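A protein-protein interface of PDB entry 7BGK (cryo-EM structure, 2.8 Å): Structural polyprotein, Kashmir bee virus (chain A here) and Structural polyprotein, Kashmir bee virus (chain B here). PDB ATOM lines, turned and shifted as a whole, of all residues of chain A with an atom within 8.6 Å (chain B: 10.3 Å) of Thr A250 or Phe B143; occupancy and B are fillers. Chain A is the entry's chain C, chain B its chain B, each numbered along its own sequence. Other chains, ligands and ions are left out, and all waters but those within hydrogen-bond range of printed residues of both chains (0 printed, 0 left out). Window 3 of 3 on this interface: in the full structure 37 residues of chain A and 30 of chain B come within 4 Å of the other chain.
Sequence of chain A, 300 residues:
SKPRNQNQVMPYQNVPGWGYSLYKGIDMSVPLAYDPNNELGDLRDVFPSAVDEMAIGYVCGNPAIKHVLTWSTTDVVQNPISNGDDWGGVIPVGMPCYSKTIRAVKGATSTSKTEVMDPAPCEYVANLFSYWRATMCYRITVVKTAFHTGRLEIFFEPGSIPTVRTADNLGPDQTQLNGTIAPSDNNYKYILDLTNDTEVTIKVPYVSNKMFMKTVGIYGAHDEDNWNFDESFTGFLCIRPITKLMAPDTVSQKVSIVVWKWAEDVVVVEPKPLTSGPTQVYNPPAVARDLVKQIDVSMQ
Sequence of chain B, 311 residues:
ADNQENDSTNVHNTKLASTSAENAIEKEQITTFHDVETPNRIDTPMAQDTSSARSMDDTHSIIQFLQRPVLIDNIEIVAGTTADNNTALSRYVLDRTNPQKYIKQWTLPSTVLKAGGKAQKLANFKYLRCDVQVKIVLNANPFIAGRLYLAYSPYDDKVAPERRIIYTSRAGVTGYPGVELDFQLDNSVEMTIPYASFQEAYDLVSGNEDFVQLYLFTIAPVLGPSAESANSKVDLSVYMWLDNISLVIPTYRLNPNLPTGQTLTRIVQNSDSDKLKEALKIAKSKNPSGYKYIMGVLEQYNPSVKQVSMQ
O of Ala B145 lies within hydrogen-bond range of N of Leu B223, at 2.9 Å. The backbone carbonyl oxygen (O) of His A148 lies within hydrogen-bond range of the side-chain amino group (NZ) of Lys A144, at 3.3 Å. O of Ser A252 is in hydrogen-bond range of NE2 of His A148. The side-chain amide nitrogen (NE2) of Gln B184 is in hydrogen-bond range of the backbone carbonyl oxygen (O) of Ala B140. The side-chain hydroxyl of Thr A145 sits close to the backbone NH of Phe A147 (3.1 Å). The side-chain amide nitrogen (NE2) of Gln B184 is in hydrogen-bond range of the backbone carbonyl oxygen (O) of Ile B144 (2.5 Å).
Among the printed residues, pairs that only touch across the chains: Lys A144 with Ala B145, Lys A144 with Gln B184, Thr A145 with Pro B142, Thr A145 with Ile B144, Thr A145 with Ala B145, Phe A147 with Pro B142, Phe A147 with Phe B143, Thr A250 with Phe B143, Thr A250 with Pro B225, Val A251 with Phe B143, Val A251 with Pro B225, Ser A252 with Leu B223 and Ser A252 with Gly B224.
Of the printed residues of chain B, Lys A144 touches Ala B145 and Gln B184. Of the printed residues of chain B, Thr A145 touches Pro B142 (3.3 Å), Ile B144 (3.9 Å) and Ala B145 (3.8 Å). No residue of chain B comes within 4 Å of Pro A248. No residue of chain B comes within 4 Å of Asp A249. Thr A250 touches just these residues of chain B: Phe B143 and Pro B225. Val A251 touches just these residues of chain B: Phe B143 (3.5 Å) and Pro B225 (3.8 Å). Phe B143 touches three residues of chain A. Of the printed residues of chain A, Ile B144 touches Thr A145 (3.9 Å). Phe B183 touches none of the printed residues of chain A. Pro B221 touches none of the printed residues of chain A. Of the printed residues of chain A, Leu B223 touches Ser A252. Printed residues of chain A within 4 Å of Gly B224: Ser A252. The nearest residue of chain B that does not touch Thr A250 is Gly B224 (5.8 Å). The nearest residue of chain A that does not touch Phe B143 is Thr A145 (4.1 Å). The nearest printed residue of chain A that does not touch Gln B184 is Thr A145 (4.3 Å).
Of the 24 printed residues of chain B, 8 touch a printed residue of chain A. Hydrophobic or aromatic side chains of chain B within 4 Å of the printed part of chain A: Pro B142, Phe B143, Ala B145, Leu B223 and Pro B225. Of the 12 printed residues of chain A, 6 touch a printed residue of chain B. Printed residues of chain A that touch a printed residue of chain B: Lys A144, Thr A145, Phe A147, Thr A250, Val A251 and Ser A252. Among the printed residues, 13 pairs touch across the chains. Among the printed residues, no Asp or Glu carboxylate lies within 4 Å of a Lys or Arg side-chain nitrogen of the other chain.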
ATOM      1  N   LYS A 144      -4.733   8.346  -4.554  1.00  0.00           N
ATOM      2  CA  LYS A 144      -6.096   7.889  -4.736  1.00  0.00           C
ATOM      3  C   LYS A 144      -6.728   7.688  -3.366  1.00  0.00           C
ATOM      4  O   LYS A 144      -6.209   8.154  -2.348  1.00  0.00           O
ATOM      5  CB  LYS A 144      -6.120   6.613  -5.579  1.00  0.00           C
ATOM      6  CG  LYS A 144      -5.448   5.442  -4.929  1.00  0.00           C
ATOM      7  CD  LYS A 144      -5.678   4.186  -5.685  1.00  0.00           C
ATOM      8  CE  LYS A 144      -5.562   2.999  -4.778  1.00  0.00           C
ATOM      9  NZ  LYS A 144      -6.822   2.702  -4.063  1.00  0.00           N
ATOM     10  N   THR A 145      -7.858   6.990  -3.345  1.00  0.00           N
ATOM     11  CA  THR A 145      -8.580   6.667  -2.129  1.00  0.00           C
ATOM     12  C   THR A 145      -8.895   5.180  -2.121  1.00  0.00           C
ATOM     13  O   THR A 145      -8.533   4.438  -3.036  1.00  0.00           O
ATOM     14  CB  THR A 145      -9.875   7.479  -2.001  1.00  0.00           C
ATOM     15  OG1 THR A 145     -10.840   6.991  -2.934  1.00  0.00           O
ATOM     16  CG2 THR A 145      -9.630   8.919  -2.281  1.00  0.00           C
ATOM     17  N   ALA A 146      -9.581   4.747  -1.069  1.00  0.00           N
ATOM     18  CA  ALA A 146     -10.057   3.378  -0.967  1.00  0.00           C
ATOM     19  C   ALA A 146     -11.165   3.055  -1.951  1.00  0.00           C
ATOM     20  O   ALA A 146     -11.615   1.905  -1.983  1.00  0.00           O
ATOM     21  CB  ALA A 146     -10.545   3.116   0.452  1.00  0.00           C
ATOM     22  N   PHE A 147     -11.612   4.023  -2.748  1.00  0.00           N
ATOM     23  CA  PHE A 147     -12.739   3.841  -3.643  1.00  0.00           C
ATOM     24  C   PHE A 147     -12.373   3.962  -5.110  1.00  0.00           C
ATOM     25  O   PHE A 147     -13.220   3.687  -5.964  1.00  0.00           O
ATOM     26  CB  PHE A 147     -13.834   4.855  -3.299  1.00  0.00           C
ATOM     27  CG  PHE A 147     -14.122   4.934  -1.837  1.00  0.00           C
ATOM     28  CD1 PHE A 147     -15.043   4.095  -1.253  1.00  0.00           C
ATOM     29  CD2 PHE A 147     -13.441   5.825  -1.038  1.00  0.00           C
ATOM     30  CE1 PHE A 147     -15.290   4.160   0.094  1.00  0.00           C
ATOM     31  CE2 PHE A 147     -13.686   5.891   0.305  1.00  0.00           C
ATOM     32  CZ  PHE A 147     -14.609   5.059   0.873  1.00  0.00           C
ATOM     33  N   HIS A 148     -11.151   4.372  -5.424  1.00  0.00           N
ATOM     34  CA  HIS A 148     -10.621   4.249  -6.770  1.00  0.00           C
ATOM     35  C   HIS A 148     -10.068   2.848  -6.974  1.00  0.00           C
ATOM     36  O   HIS A 148      -9.351   2.325  -6.118  1.00  0.00           O
ATOM     37  CB  HIS A 148      -9.518   5.270  -7.010  1.00  0.00           C
ATOM     38  CG  HIS A 148      -9.989   6.687  -7.023  1.00  0.00           C
ATOM     39  ND1 HIS A 148      -9.784   7.546  -5.967  1.00  0.00           N
ATOM     40  CD2 HIS A 148     -10.635   7.402  -7.971  1.00  0.00           C
ATOM     41  CE1 HIS A 148     -10.292   8.728  -6.262  1.00  0.00           C
ATOM     42  NE2 HIS A 148     -10.814   8.666  -7.473  1.00  0.00           N
ATOM     43  N   ALA A 247     -14.385   4.720 -10.601  1.00  0.00           N
ATOM     44  CA  ALA A 247     -14.500   5.712  -9.548  1.00  0.00           C
ATOM     45  C   ALA A 247     -15.949   6.155  -9.405  1.00  0.00           C
ATOM     46  O   ALA A 247     -16.583   6.515 -10.404  1.00  0.00           O
ATOM     47  CB  ALA A 247     -13.601   6.907  -9.843  1.00  0.00           C
ATOM     48  N   PRO A 248     -16.513   6.139  -8.202  1.00  0.00           N
ATOM     49  CA  PRO A 248     -17.861   6.675  -8.017  1.00  0.00           C
ATOM     50  C   PRO A 248     -17.879   8.189  -8.140  1.00  0.00           C
ATOM     51  O   PRO A 248     -16.847   8.859  -8.213  1.00  0.00           O
ATOM     52  CB  PRO A 248     -18.233   6.224  -6.607  1.00  0.00           C
ATOM     53  CG  PRO A 248     -16.964   6.007  -5.930  1.00  0.00           C
ATOM     54  CD  PRO A 248     -15.988   5.563  -6.955  1.00  0.00           C
ATOM     55  N   ASP A 249     -19.093   8.728  -8.170  1.00  0.00           N
ATOM     56  CA  ASP A 249     -19.287  10.168  -8.219  1.00  0.00           C
ATOM     57  C   ASP A 249     -19.071  10.830  -6.866  1.00  0.00           C
ATOM     58  O   ASP A 249     -19.185  12.055  -6.769  1.00  0.00           O
ATOM     59  CB  ASP A 249     -20.691  10.477  -8.735  1.00  0.00           C
ATOM     60  CG  ASP A 249     -21.009   9.747 -10.018  1.00  0.00           C
ATOM     61  OD1 ASP A 249     -22.207   9.544 -10.309  1.00  0.00           O
ATOM     62  OD2 ASP A 249     -20.062   9.361 -10.732  1.00  0.00           O
ATOM     63  N   THR A 250     -18.760  10.054  -5.833  1.00  0.00           N
ATOM     64  CA  THR A 250     -18.470  10.575  -4.507  1.00  0.00           C
ATOM     65  C   THR A 250     -16.994  10.866  -4.299  1.00  0.00           C
ATOM     66  O   THR A 250     -16.620  11.368  -3.236  1.00  0.00           O
ATOM     67  CB  THR A 250     -18.937   9.585  -3.438  1.00  0.00           C
ATOM     68  OG1 THR A 250     -18.214   8.357  -3.575  1.00  0.00           O
ATOM     69  CG2 THR A 250     -20.411   9.311  -3.564  1.00  0.00           C
ATOM     70  N   VAL A 251     -16.152  10.566  -5.282  1.00  0.00           N
ATOM     71  CA  VAL A 251     -14.725  10.800  -5.212  1.00  0.00           C
ATOM     72  C   VAL A 251     -14.290  11.502  -6.493  1.00  0.00           C
ATOM     73  O   VAL A 251     -15.084  11.731  -7.403  1.00  0.00           O
ATOM     74  CB  VAL A 251     -13.926   9.498  -4.998  1.00  0.00           C
ATOM     75  CG1 VAL A 251     -14.310   8.836  -3.704  1.00  0.00           C
ATOM     76  CG2 VAL A 251     -14.140   8.545  -6.144  1.00  0.00           C
ATOM     77  N   SER A 252     -13.007  11.843  -6.551  1.00  0.00           N
ATOM     78  CA  SER A 252     -12.454  12.466  -7.741  1.00  0.00           C
ATOM     79  C   SER A 252     -12.510  11.511  -8.922  1.00  0.00           C
ATOM     80  O   SER A 252     -12.319  10.301  -8.778  1.00  0.00           O
ATOM     81  CB  SER A 252     -11.017  12.901  -7.484  1.00  0.00           C
ATOM     82  OG  SER A 252     -10.475  13.566  -8.603  1.00  0.00           O
ATOM     83  N   GLN A 253     -12.770  12.066 -10.103  1.00  0.00           N
ATOM     84  CA  GLN A 253     -12.754  11.310 -11.343  1.00  0.00           C
ATOM     85  C   GLN A 253     -11.369  11.235 -11.958  1.00  0.00           C
ATOM     86  O   GLN A 253     -11.239  10.907 -13.141  1.00  0.00           O
ATOM     87  CB  GLN A 253     -13.738  11.920 -12.338  1.00  0.00           C
ATOM     88  CG  GLN A 253     -15.180  11.828 -11.908  1.00  0.00           C
ATOM     89  CD  GLN A 253     -15.667  10.405 -11.791  1.00  0.00           C
ATOM     90  OE1 GLN A 253     -15.822   9.705 -12.789  1.00  0.00           O
ATOM     91  NE2 GLN A 253     -15.913   9.967 -10.566  1.00  0.00           N
ATOM     92  N   ALA B  79     -10.557  22.276  -1.895  1.00  0.00           N
ATOM     93  CA  ALA B  79     -10.406  21.836  -3.267  1.00  0.00           C
ATOM     94  C   ALA B  79     -11.087  22.806  -4.219  1.00  0.00           C
ATOM     95  O   ALA B  79     -12.050  23.492  -3.866  1.00  0.00           O
ATOM     96  CB  ALA B  79     -10.989  20.440  -3.448  1.00  0.00           C
ATOM     97  N   ASN B 139      -5.899  15.478   8.512  1.00  0.00           N
ATOM     98  CA  ASN B 139      -7.142  14.727   8.559  1.00  0.00           C
ATOM     99  C   ASN B 139      -7.956  15.037   7.316  1.00  0.00           C
ATOM    100  O   ASN B 139      -8.209  16.204   7.007  1.00  0.00           O
ATOM    101  CB  ASN B 139      -7.943  15.055   9.819  1.00  0.00           C
ATOM    102  CG  ASN B 139      -7.453  14.296  11.027  1.00  0.00           C
ATOM    103  OD1 ASN B 139      -6.698  14.822  11.841  1.00  0.00           O
ATOM    104  ND2 ASN B 139      -7.875  13.050  11.151  1.00  0.00           N
ATOM    105  N   ALA B 140      -8.357  13.984   6.608  1.00  0.00           N
ATOM    106  CA  ALA B 140      -9.111  14.106   5.373  1.00  0.00           C
ATOM    107  C   ALA B 140      -9.989  12.877   5.229  1.00  0.00           C
ATOM    108  O   ALA B 140      -9.493  11.750   5.313  1.00  0.00           O
ATOM    109  CB  ALA B 140      -8.180  14.235   4.172  1.00  0.00           C
ATOM    110  N   ASN B 141     -11.283  13.094   5.018  1.00  0.00           N
ATOM    111  CA  ASN B 141     -12.212  11.986   4.945  1.00  0.00           C
ATOM    112  C   ASN B 141     -11.771  11.011   3.857  1.00  0.00           C
ATOM    113  O   ASN B 141     -10.962  11.355   2.993  1.00  0.00           O
ATOM    114  CB  ASN B 141     -13.627  12.501   4.684  1.00  0.00           C
ATOM    115  CG  ASN B 141     -13.839  12.977   3.266  1.00  0.00           C
ATOM    116  OD1 ASN B 141     -13.139  12.578   2.347  1.00  0.00           O
ATOM    117  ND2 ASN B 141     -14.802  13.856   3.087  1.00  0.00           N
ATOM    118  N   PRO B 142     -12.285   9.779   3.881  1.00  0.00           N
ATOM    119  CA  PRO B 142     -11.790   8.764   2.943  1.00  0.00           C
ATOM    120  C   PRO B 142     -12.080   9.070   1.488  1.00  0.00           C
ATOM    121  O   PRO B 142     -11.615   8.322   0.620  1.00  0.00           O
ATOM    122  CB  PRO B 142     -12.518   7.493   3.390  1.00  0.00           C
ATOM    123  CG  PRO B 142     -13.016   7.773   4.729  1.00  0.00           C
ATOM    124  CD  PRO B 142     -13.274   9.219   4.808  1.00  0.00           C
ATOM    125  N   PHE B 143     -12.832  10.125   1.190  1.00  0.00           N
ATOM    126  CA  PHE B 143     -13.185  10.474  -0.176  1.00  0.00           C
ATOM    127  C   PHE B 143     -12.334  11.595  -0.749  1.00  0.00           C
ATOM    128  O   PHE B 143     -12.590  12.032  -1.874  1.00  0.00           O
ATOM    129  CB  PHE B 143     -14.658  10.862  -0.248  1.00  0.00           C
ATOM    130  CG  PHE B 143     -15.589   9.785   0.207  1.00  0.00           C
ATOM    131  CD1 PHE B 143     -16.107   8.878  -0.691  1.00  0.00           C
ATOM    132  CD2 PHE B 143     -15.952   9.682   1.530  1.00  0.00           C
ATOM    133  CE1 PHE B 143     -16.963   7.895  -0.280  1.00  0.00           C
ATOM    134  CE2 PHE B 143     -16.809   8.693   1.946  1.00  0.00           C
ATOM    135  CZ  PHE B 143     -17.314   7.801   1.036  1.00  0.00           C
ATOM    136  N   ILE B 144     -11.336  12.069  -0.012  1.00  0.00           N
ATOM    137  CA  ILE B 144     -10.432  13.113  -0.472  1.00  0.00           C
ATOM    138  C   ILE B 144      -9.043  12.518  -0.611  1.00  0.00           C
ATOM    139  O   ILE B 144      -8.606  11.725   0.229  1.00  0.00           O
ATOM    140  CB  ILE B 144     -10.417  14.331   0.473  1.00  0.00           C
ATOM    141  CG1 ILE B 144     -11.828  14.862   0.704  1.00  0.00           C
ATOM    142  CG2 ILE B 144      -9.540  15.424  -0.076  1.00  0.00           C
ATOM    143  CD1 ILE B 144     -12.547  15.285  -0.528  1.00  0.00           C
ATOM    144  N   ALA B 145      -8.352  12.906  -1.676  1.00  0.00           N
ATOM    145  CA  ALA B 145      -7.008  12.447  -1.960  1.00  0.00           C
ATOM    146  C   ALA B 145      -6.097  13.645  -2.166  1.00  0.00           C
ATOM    147  O   ALA B 145      -6.546  14.788  -2.277  1.00  0.00           O
ATOM    148  CB  ALA B 145      -6.981  11.539  -3.187  1.00  0.00           C
ATOM    149  N   GLY B 146      -4.807  13.371  -2.215  1.00  0.00           N
ATOM    150  CA  GLY B 146      -3.819  14.417  -2.364  1.00  0.00           C
ATOM    151  C   GLY B 146      -2.489  13.979  -1.810  1.00  0.00           C
ATOM    152  O   GLY B 146      -2.355  12.921  -1.201  1.00  0.00           O
ATOM    153  N   ASP B 182       0.876  11.752   2.104  1.00  0.00           N
ATOM    154  CA  ASP B 182      -0.372  11.426   1.439  1.00  0.00           C
ATOM    155  C   ASP B 182      -1.522  11.454   2.434  1.00  0.00           C
ATOM    156  O   ASP B 182      -1.355  11.154   3.617  1.00  0.00           O
ATOM    157  CB  ASP B 182      -0.283  10.053   0.780  1.00  0.00           C
ATOM    158  CG  ASP B 182      -1.201   9.913  -0.418  1.00  0.00           C
ATOM    159  OD1 ASP B 182      -2.319  10.465  -0.386  1.00  0.00           O
ATOM    160  OD2 ASP B 182      -0.805   9.247  -1.395  1.00  0.00           O
ATOM    161  N   PHE B 183      -2.703  11.811   1.934  1.00  0.00           N
ATOM    162  CA  PHE B 183      -3.848  11.996   2.814  1.00  0.00           C
ATOM    163  C   PHE B 183      -4.383  10.663   3.321  1.00  0.00           C
ATOM    164  O   PHE B 183      -4.805  10.558   4.477  1.00  0.00           O
ATOM    165  CB  PHE B 183      -4.941  12.775   2.084  1.00  0.00           C
ATOM    166  CG  PHE B 183      -4.542  14.169   1.688  1.00  0.00           C
ATOM    167  CD1 PHE B 183      -3.307  14.686   2.021  1.00  0.00           C
ATOM    168  CD2 PHE B 183      -5.412  14.964   0.977  1.00  0.00           C
ATOM    169  CE1 PHE B 183      -2.958  15.955   1.651  1.00  0.00           C
ATOM    170  CE2 PHE B 183      -5.058  16.232   0.606  1.00  0.00           C
ATOM    171  CZ  PHE B 183      -3.834  16.726   0.944  1.00  0.00           C
ATOM    172  N   GLN B 184      -4.373   9.637   2.475  1.00  0.00           N
ATOM    173  CA  GLN B 184      -4.952   8.346   2.815  1.00  0.00           C
ATOM    174  C   GLN B 184      -3.921   7.299   3.206  1.00  0.00           C
ATOM    175  O   GLN B 184      -4.306   6.198   3.608  1.00  0.00           O
ATOM    176  CB  GLN B 184      -5.786   7.818   1.644  1.00  0.00           C
ATOM    177  CG  GLN B 184      -6.981   8.676   1.268  1.00  0.00           C
ATOM    178  CD  GLN B 184      -7.744   9.197   2.458  1.00  0.00           C
ATOM    179  OE1 GLN B 184      -7.959   8.487   3.437  1.00  0.00           O
ATOM    180  NE2 GLN B 184      -8.165  10.445   2.378  1.00  0.00           N
ATOM    181  N   PRO B 221      -2.797  18.473  -5.880  1.00  0.00           N
ATOM    182  CA  PRO B 221      -3.803  19.229  -5.133  1.00  0.00           C
ATOM    183  C   PRO B 221      -4.902  18.327  -4.597  1.00  0.00           C
ATOM    184  O   PRO B 221      -5.011  17.147  -4.933  1.00  0.00           O
ATOM    185  CB  PRO B 221      -4.336  20.219  -6.169  1.00  0.00           C
ATOM    186  CG  PRO B 221      -4.053  19.603  -7.458  1.00  0.00           C
ATOM    187  CD  PRO B 221      -2.781  18.862  -7.297  1.00  0.00           C
ATOM    188  N   VAL B 222      -5.734  18.913  -3.740  1.00  0.00           N
ATOM    189  CA  VAL B 222      -6.832  18.169  -3.137  1.00  0.00           C
ATOM    190  C   VAL B 222      -7.753  17.675  -4.239  1.00  0.00           C
ATOM    191  O   VAL B 222      -8.371  18.469  -4.959  1.00  0.00           O
ATOM    192  CB  VAL B 222      -7.584  19.032  -2.123  1.00  0.00           C
ATOM    193  CG1 VAL B 222      -8.649  18.227  -1.438  1.00  0.00           C
ATOM    194  CG2 VAL B 222      -6.640  19.597  -1.099  1.00  0.00           C
ATOM    195  N   LEU B 223      -7.847  16.358  -4.380  1.00  0.00           N
ATOM    196  CA  LEU B 223      -8.703  15.727  -5.373  1.00  0.00           C
ATOM    197  C   LEU B 223     -10.003  15.315  -4.700  1.00  0.00           C
ATOM    198  O   LEU B 223     -10.024  14.382  -3.892  1.00  0.00           O
ATOM    199  CB  LEU B 223      -8.012  14.522  -5.998  1.00  0.00           C
ATOM    200  CG  LEU B 223      -6.633  14.771  -6.590  1.00  0.00           C
ATOM    201  CD1 LEU B 223      -5.999  13.461  -6.934  1.00  0.00           C
ATOM    202  CD2 LEU B 223      -6.727  15.646  -7.808  1.00  0.00           C
ATOM    203  N   GLY B 224     -11.082  16.009  -5.035  1.00  0.00           N
ATOM    204  CA  GLY B 224     -12.381  15.706  -4.496  1.00  0.00           C
ATOM    205  C   GLY B 224     -13.437  15.630  -5.574  1.00  0.00           C
ATOM    206  O   GLY B 224     -13.161  15.813  -6.763  1.00  0.00           O
ATOM    207  N   PRO B 225     -14.671  15.347  -5.172  1.00  0.00           N
ATOM    208  CA  PRO B 225     -15.763  15.252  -6.142  1.00  0.00           C
ATOM    209  C   PRO B 225     -15.834  16.471  -7.050  1.00  0.00           C
ATOM    210  O   PRO B 225     -15.417  17.571  -6.686  1.00  0.00           O
ATOM    211  CB  PRO B 225     -17.006  15.140  -5.257  1.00  0.00           C
ATOM    212  CG  PRO B 225     -16.517  14.549  -4.007  1.00  0.00           C
ATOM    213  CD  PRO B 225     -15.116  15.017  -3.810  1.00  0.00           C
ATOM    214  N   SER B 226     -16.379  16.258  -8.249  1.00  0.00           N
ATOM    215  CA  SER B 226     -16.630  17.368  -9.160  1.00  0.00           C
ATOM    216  C   SER B 226     -17.644  18.338  -8.574  1.00  0.00           C
ATOM    217  O   SER B 226     -17.501  19.558  -8.712  1.00  0.00           O
ATOM    218  CB  SER B 226     -17.126  16.836 -10.503  1.00  0.00           C
ATOM    219  OG  SER B 226     -16.138  16.051 -11.144  1.00  0.00           O
ATOM    220  N   ALA B 227     -18.671  17.814  -7.915  1.00  0.00           N
ATOM    221  CA  ALA B 227     -19.719  18.645  -7.345  1.00  0.00           C
ATOM    222  C   ALA B 227     -19.150  19.518  -6.236  1.00  0.00           C
ATOM    223  O   ALA B 227     -18.572  19.010  -5.270  1.00  0.00           O
ATOM    224  CB  ALA B 227     -20.848  17.771  -6.814  1.00  0.00           C
ATOM    225  N   SER B 229     -18.582  21.461  -2.984  1.00  0.00           N
ATOM    226  CA  SER B 229     -19.011  21.089  -1.648  1.00  0.00           C
ATOM    227  C   SER B 229     -18.030  21.672  -0.648  1.00  0.00           C
ATOM    228  O   SER B 229     -16.828  21.731  -0.911  1.00  0.00           O
ATOM    229  CB  SER B 229     -19.084  19.569  -1.492  1.00  0.00           C
ATOM    230  OG  SER B 229     -19.687  19.204  -0.266  1.00  0.00           O
ATOM    231  N   ASN B 231     -17.236  20.207   1.938  1.00  0.00           N
ATOM    232  CA  ASN B 231     -16.605  19.075   2.592  1.00  0.00           C
ATOM    233  C   ASN B 231     -15.352  18.590   1.888  1.00  0.00           C
ATOM    234  O   ASN B 231     -14.571  17.844   2.492  1.00  0.00           O
ATOM    235  CB  ASN B 231     -17.605  17.921   2.688  1.00  0.00           C
ATOM    236  CG  ASN B 231     -18.835  18.283   3.482  1.00  0.00           C
ATOM    237  OD1 ASN B 231     -19.957  18.138   3.006  1.00  0.00           O
ATOM    238  ND2 ASN B 231     -18.632  18.759   4.700  1.00  0.00           N
ATOM    239  N   SER B 232     -15.147  18.984   0.634  1.00  0.00           N
ATOM    240  CA  SER B 232     -13.955  18.598  -0.119  1.00  0.00           C
ATOM    241  C   SER B 232     -12.808  19.506   0.299  1.00  0.00           C
ATOM    242  O   SER B 232     -12.520  20.524  -0.330  1.00  0.00           O
ATOM    243  CB  SER B 232     -14.213  18.659  -1.615  1.00  0.00           C
ATOM    244  OG  SER B 232     -15.290  17.811  -1.963  1.00  0.00           O
ATOM    245  N   LYS B 233     -12.141  19.122   1.382  1.00  0.00           N
ATOM    246  CA  LYS B 233     -11.082  19.928   1.965  1.00  0.00           C
ATOM    247  C   LYS B 233     -10.286  19.051   2.913  1.00  0.00           C
ATOM    248  O   LYS B 233     -10.654  17.907   3.192  1.00  0.00           O
ATOM    249  CB  LYS B 233     -11.657  21.141   2.698  1.00  0.00           C
ATOM    250  CG  LYS B 233     -12.535  20.783   3.873  1.00  0.00           C
ATOM    251  CD  LYS B 233     -13.137  22.002   4.504  1.00  0.00           C
ATOM    252  CE  LYS B 233     -13.870  21.652   5.777  1.00  0.00           C
ATOM    253  NZ  LYS B 233     -14.667  22.798   6.285  1.00  0.00           N
ATOM    254  N   VAL B 234      -9.182  19.604   3.405  1.00  0.00           N
ATOM    255  CA  VAL B 234      -8.383  18.958   4.433  1.00  0.00           C
ATOM    256  C   VAL B 234      -7.950  20.007   5.443  1.00  0.00           C
ATOM    257  O   VAL B 234      -7.768  21.180   5.110  1.00  0.00           O
ATOM    258  CB  VAL B 234      -7.163  18.224   3.835  1.00  0.00           C
ATOM    259  CG1 VAL B 234      -7.608  17.321   2.734  1.00  0.00           C
ATOM    260  CG2 VAL B 234      -6.149  19.197   3.310  1.00  0.00           C
